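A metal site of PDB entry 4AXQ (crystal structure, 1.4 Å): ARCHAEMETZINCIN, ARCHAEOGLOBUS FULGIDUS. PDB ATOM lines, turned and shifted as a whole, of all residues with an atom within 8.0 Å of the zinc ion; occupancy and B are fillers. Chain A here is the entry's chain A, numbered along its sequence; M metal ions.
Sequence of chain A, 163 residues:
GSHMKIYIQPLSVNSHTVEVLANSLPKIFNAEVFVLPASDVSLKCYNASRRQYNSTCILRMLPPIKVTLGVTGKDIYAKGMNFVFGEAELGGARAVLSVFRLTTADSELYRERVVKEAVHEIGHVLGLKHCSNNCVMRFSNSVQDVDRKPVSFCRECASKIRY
The zinc ion is bound by the side-chain sulfur of Cys 157, the side-chain sulfur of Cys 131, the side-chain sulfur of Cys 135 and the side-chain sulfur of Cys 154.
Four residues have an atom within 4 Å of the zinc ion: Cys 131, Cys 135, Cys 154 and Cys 157.
The backbone NH (N) of Cys 131 sits at hydrogen-bond distance from the backbone carbonyl oxygen (O) of Met 137 (3.1 Å). The side-chain sulfur of Cys 131 lies close to the backbone NH of Asn 133 (3.4 Å). SG of Cys 135 sits close to N of Met 137. The side-chain sulfur of Cys 154 sits close to the side-chain amide nitrogen of Asn 133 (3.5 Å). The side-chain sulfur (SG) of Cys 154 sits close to the backbone NH (N) of Glu 156 (3.5 Å).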
ATOM      1  N   LEU A 128      -4.008  10.147   7.801  1.00  0.00           N
ATOM      2  CA  LEU A 128      -4.101   9.784   6.382  1.00  0.00           C
ATOM      3  C   LEU A 128      -3.135  10.581   5.532  1.00  0.00           C
ATOM      4  O   LEU A 128      -3.100  11.795   5.614  1.00  0.00           O
ATOM      5  CB  LEU A 128      -5.503   9.992   5.842  1.00  0.00           C
ATOM      6  CG  LEU A 128      -6.604   9.146   6.488  1.00  0.00           C
ATOM      7  CD1 LEU A 128      -7.959   9.530   5.907  1.00  0.00           C
ATOM      8  CD2 LEU A 128      -6.343   7.662   6.316  1.00  0.00           C
ATOM      9  N   LYS A 129      -2.366   9.882   4.715  1.00  0.00           N
ATOM     10  CA  LYS A 129      -1.542  10.507   3.693  1.00  0.00           C
ATOM     11  C   LYS A 129      -2.375  10.814   2.441  1.00  0.00           C
ATOM     12  O   LYS A 129      -3.532  10.394   2.326  1.00  0.00           O
ATOM     13  CB  LYS A 129      -0.389   9.565   3.325  1.00  0.00           C
ATOM     14  CG  LYS A 129       0.494   9.215   4.533  1.00  0.00           C
ATOM     15  CD  LYS A 129       1.604   8.231   4.135  1.00  0.00           C
ATOM     16  CE  LYS A 129       2.548   7.933   5.298  1.00  0.00           C
ATOM     17  NZ  LYS A 129       1.871   7.183   6.409  1.00  0.00           N
ATOM     18  N   HIS A 130      -1.805  11.553   1.503  1.00  0.00           N
ATOM     19  CA  HIS A 130      -2.483  11.767   0.244  1.00  0.00           C
ATOM     20  C   HIS A 130      -2.742  10.444  -0.465  1.00  0.00           C
ATOM     21  O   HIS A 130      -1.965   9.502  -0.338  1.00  0.00           O
ATOM     22  CB  HIS A 130      -1.724  12.738  -0.642  1.00  0.00           C
ATOM     23  CG  HIS A 130      -1.833  14.154  -0.181  1.00  0.00           C
ATOM     24  ND1 HIS A 130      -0.911  15.115  -0.518  1.00  0.00           N
ATOM     25  CD2 HIS A 130      -2.776  14.780   0.569  1.00  0.00           C
ATOM     26  CE1 HIS A 130      -1.262  16.270   0.018  1.00  0.00           C
ATOM     27  NE2 HIS A 130      -2.387  16.088   0.693  1.00  0.00           N
ATOM     28  N   CYS A 131      -3.827  10.409  -1.221  1.00  0.00           N
ATOM     29  CA  CYS A 131      -4.365   9.176  -1.766  1.00  0.00           C
ATOM     30  C   CYS A 131      -4.459   9.350  -3.273  1.00  0.00           C
ATOM     31  O   CYS A 131      -4.711  10.464  -3.738  1.00  0.00           O
ATOM     32  CB  CYS A 131      -5.761   8.960  -1.170  1.00  0.00           C
ATOM     33  SG  CYS A 131      -6.585   7.464  -1.720  1.00  0.00           S
ATOM     34  N   SER A 132      -4.247   8.273  -4.013  1.00  0.00           N
ATOM     35  CA  SER A 132      -4.302   8.335  -5.466  1.00  0.00           C
ATOM     36  C   SER A 132      -5.658   7.913  -6.011  1.00  0.00           C
ATOM     37  O   SER A 132      -5.898   8.018  -7.230  1.00  0.00           O
ATOM     38  CB  SER A 132      -3.230   7.439  -6.078  1.00  0.00           C
ATOM     39  OG  SER A 132      -3.452   6.079  -5.740  1.00  0.00           O
ATOM     40  N   ASN A 133      -6.532   7.411  -5.144  1.00  0.00           N
ATOM     41  CA  ASN A 133      -7.867   7.001  -5.570  1.00  0.00           C
ATOM     42  C   ASN A 133      -8.787   8.191  -5.755  1.00  0.00           C
ATOM     43  O   ASN A 133      -8.391   9.335  -5.507  1.00  0.00           O
ATOM     44  CB  ASN A 133      -8.494   6.039  -4.550  1.00  0.00           C
ATOM     45  CG  ASN A 133      -7.789   4.683  -4.492  1.00  0.00           C
ATOM     46  OD1 ASN A 133      -7.310   4.179  -5.506  1.00  0.00           O
ATOM     47  ND2 ASN A 133      -7.713   4.102  -3.302  1.00  0.00           N
ATOM     48  N   ASN A 134     -10.004   7.918  -6.189  1.00  0.00           N
ATOM     49  CA  ASN A 134     -11.059   8.931  -6.236  1.00  0.00           C
ATOM     50  C   ASN A 134     -11.483   9.196  -4.805  1.00  0.00           C
ATOM     51  O   ASN A 134     -12.320   8.476  -4.258  1.00  0.00           O
ATOM     52  CB  ASN A 134     -12.232   8.435  -7.081  1.00  0.00           C
ATOM     53  CG  ASN A 134     -13.231   9.529  -7.385  1.00  0.00           C
ATOM     54  OD1 ASN A 134     -12.851  10.678  -7.627  1.00  0.00           O
ATOM     55  ND2 ASN A 134     -14.504   9.182  -7.375  1.00  0.00           N
ATOM     56  N   CYS A 135     -10.915  10.228  -4.191  1.00  0.00           N
ATOM     57  CA  CYS A 135     -10.923  10.314  -2.740  1.00  0.00           C
ATOM     58  C   CYS A 135     -10.691  11.743  -2.337  1.00  0.00           C
ATOM     59  O   CYS A 135      -9.917  12.449  -2.964  1.00  0.00           O
ATOM     60  CB  CYS A 135      -9.801   9.428  -2.187  1.00  0.00           C
ATOM     61  SG  CYS A 135      -9.706   9.312  -0.379  1.00  0.00           S
ATOM     62  N   VAL A 136     -11.289  12.139  -1.225  1.00  0.00           N
ATOM     63  CA  VAL A 136     -11.107  13.472  -0.698  1.00  0.00           C
ATOM     64  C   VAL A 136      -9.644  13.703  -0.254  1.00  0.00           C
ATOM     65  O   VAL A 136      -9.197  14.839  -0.129  1.00  0.00           O
ATOM     66  CB  VAL A 136     -12.067  13.689   0.499  1.00  0.00           C
ATOM     67  CG1 VAL A 136     -11.707  12.810   1.684  1.00  0.00           C
ATOM     68  CG2 VAL A 136     -12.159  15.147   0.867  1.00  0.00           C
ATOM     69  N   MET A 137      -8.899  12.620  -0.047  1.00  0.00           N
ATOM     70  CA  MET A 137      -7.506  12.751   0.345  1.00  0.00           C
ATOM     71  C   MET A 137      -6.566  12.963  -0.834  1.00  0.00           C
ATOM     72  O   MET A 137      -5.362  13.024  -0.635  1.00  0.00           O
ATOM     73  CB  MET A 137      -7.038  11.568   1.206  1.00  0.00           C
ATOM     74  CG  MET A 137      -7.708  11.500   2.575  1.00  0.00           C
ATOM     75  SD  MET A 137      -7.629  13.049   3.521  1.00  0.00           S
ATOM     76  CE  MET A 137      -5.859  13.408   3.545  1.00  0.00           C
ATOM     77  N   ARG A 138      -7.114  13.100  -2.031  1.00  0.00           N
ATOM     78  CA  ARG A 138      -6.291  13.523  -3.165  1.00  0.00           C
ATOM     79  C   ARG A 138      -5.695  14.894  -2.835  1.00  0.00           C
ATOM     80  O   ARG A 138      -6.372  15.727  -2.225  1.00  0.00           O
ATOM     81  CB  ARG A 138      -7.122  13.628  -4.446  1.00  0.00           C
ATOM     82  CG  ARG A 138      -7.237  12.345  -5.253  1.00  0.00           C
ATOM     83  CD  ARG A 138      -7.640  12.648  -6.707  1.00  0.00           C
ATOM     84  NE  ARG A 138      -7.873  11.442  -7.496  1.00  0.00           N
ATOM     85  CZ  ARG A 138      -6.911  10.687  -8.021  1.00  0.00           C
ATOM     86  NH1 ARG A 138      -5.639  10.996  -7.845  1.00  0.00           N
ATOM     87  NH2 ARG A 138      -7.231   9.612  -8.724  1.00  0.00           N
ATOM     88  N   SER A 152     -16.010  12.287  -0.256  1.00  0.00           N
ATOM     89  CA  SER A 152     -15.971  11.054   0.522  1.00  0.00           C
ATOM     90  C   SER A 152     -14.582  10.456   0.555  1.00  0.00           C
ATOM     91  O   SER A 152     -13.787  10.643  -0.372  1.00  0.00           O
ATOM     92  CB  SER A 152     -16.946  10.046  -0.083  1.00  0.00           C
ATOM     93  OG  SER A 152     -16.746   9.936  -1.480  1.00  0.00           O
ATOM     94  N   PHE A 153     -14.289   9.743   1.630  1.00  0.00           N
ATOM     95  CA  PHE A 153     -13.129   8.878   1.668  1.00  0.00           C
ATOM     96  C   PHE A 153     -13.350   7.620   0.810  1.00  0.00           C
ATOM     97  O   PHE A 153     -14.426   7.008   0.833  1.00  0.00           O
ATOM     98  CB  PHE A 153     -12.817   8.477   3.105  1.00  0.00           C
ATOM     99  CG  PHE A 153     -12.453   9.645   3.989  1.00  0.00           C
ATOM    100  CD1 PHE A 153     -11.205  10.210   3.941  1.00  0.00           C
ATOM    101  CD2 PHE A 153     -13.353  10.151   4.909  1.00  0.00           C
ATOM    102  CE1 PHE A 153     -10.872  11.278   4.756  1.00  0.00           C
ATOM    103  CE2 PHE A 153     -13.017  11.215   5.733  1.00  0.00           C
ATOM    104  CZ  PHE A 153     -11.768  11.778   5.647  1.00  0.00           C
ATOM    105  N   CYS A 154     -12.300   7.235   0.090  1.00  0.00           N
ATOM    106  CA  CYS A 154     -12.292   5.957  -0.618  1.00  0.00           C
ATOM    107  C   CYS A 154     -12.332   4.818   0.391  1.00  0.00           C
ATOM    108  O   CYS A 154     -12.162   5.021   1.592  1.00  0.00           O
ATOM    109  CB  CYS A 154     -11.075   5.829  -1.529  1.00  0.00           C
ATOM    110  SG  CYS A 154      -9.552   5.455  -0.694  1.00  0.00           S
ATOM    111  N   ARG A 155     -12.567   3.604  -0.084  1.00  0.00           N
ATOM    112  CA  ARG A 155     -12.688   2.492   0.852  1.00  0.00           C
ATOM    113  C   ARG A 155     -11.408   2.268   1.651  1.00  0.00           C
ATOM    114  O   ARG A 155     -11.473   1.877   2.822  1.00  0.00           O
ATOM    115  CB  ARG A 155     -13.142   1.216   0.127  1.00  0.00           C
ATOM    116  CG  ARG A 155     -12.072   0.531  -0.671  1.00  0.00           C
ATOM    117  CD  ARG A 155     -12.635  -0.734  -1.321  1.00  0.00           C
ATOM    118  NE  ARG A 155     -11.617  -1.772  -1.492  1.00  0.00           N
ATOM    119  CZ  ARG A 155     -11.267  -2.637  -0.550  1.00  0.00           C
ATOM    120  NH1 ARG A 155     -11.827  -2.602   0.649  1.00  0.00           N
ATOM    121  NH2 ARG A 155     -10.333  -3.556  -0.815  1.00  0.00           N
ATOM    122  N   GLU A 156     -10.242   2.528   1.063  1.00  0.00           N
ATOM    123  CA  GLU A 156      -8.962   2.345   1.751  1.00  0.00           C
ATOM    124  C   GLU A 156      -8.778   3.350   2.885  1.00  0.00           C
ATOM    125  O   GLU A 156      -8.385   2.976   4.000  1.00  0.00           O
ATOM    126  CB  GLU A 156      -7.798   2.435   0.778  1.00  0.00           C
ATOM    127  CG  GLU A 156      -7.779   1.333  -0.275  1.00  0.00           C
ATOM    128  CD  GLU A 156      -6.803   1.589  -1.407  1.00  0.00           C
ATOM    129  OE1 GLU A 156      -5.720   2.194  -1.158  1.00  0.00           O
ATOM    130  OE2 GLU A 156      -7.147   1.230  -2.551  1.00  0.00           O
ATOM    131  N   CYS A 157      -9.100   4.612   2.617  1.00  0.00           N
ATOM    132  CA  CYS A 157      -8.967   5.641   3.627  1.00  0.00           C
ATOM    133  C   CYS A 157     -10.033   5.500   4.715  1.00  0.00           C
ATOM    134  O   CYS A 157      -9.753   5.698   5.892  1.00  0.00           O
ATOM    135  CB  CYS A 157      -9.041   7.026   2.985  1.00  0.00           C
ATOM    136  SG  CYS A 157      -7.593   7.410   1.962  1.00  0.00           S
ATOM    137  N   ALA A 158     -11.257   5.159   4.318  1.00  0.00           N
ATOM    138  CA  ALA A 158     -12.321   4.954   5.297  1.00  0.00           C
ATOM    139  C   ALA A 158     -11.923   3.854   6.270  1.00  0.00           C
ATOM    140  O   ALA A 158     -12.202   3.960   7.466  1.00  0.00           O
ATOM    141  CB  ALA A 158     -13.604   4.603   4.615  1.00  0.00           C
ATOM    142  N   LYS A 160      -8.861   2.996   7.152  1.00  0.00           N
ATOM    143  CA  LYS A 160      -7.791   3.470   8.027  1.00  0.00           C
ATOM    144  C   LYS A 160      -8.302   4.375   9.146  1.00  0.00           C
ATOM    145  O   LYS A 160      -7.712   4.424  10.222  1.00  0.00           O
ATOM    146  CB  LYS A 160      -6.717   4.198   7.204  1.00  0.00           C
ATOM    147  CG  LYS A 160      -5.938   3.258   6.285  1.00  0.00           C
ATOM    148  CD  LYS A 160      -4.823   3.985   5.567  1.00  0.00           C
ATOM    149  CE  LYS A 160      -3.980   3.018   4.740  1.00  0.00           C
ATOM    150  NZ  LYS A 160      -4.778   2.330   3.695  1.00  0.00           N
HETATM  151 ZN    ZN M   1      -8.343   7.448  -0.217  1.00  0.00          ZN
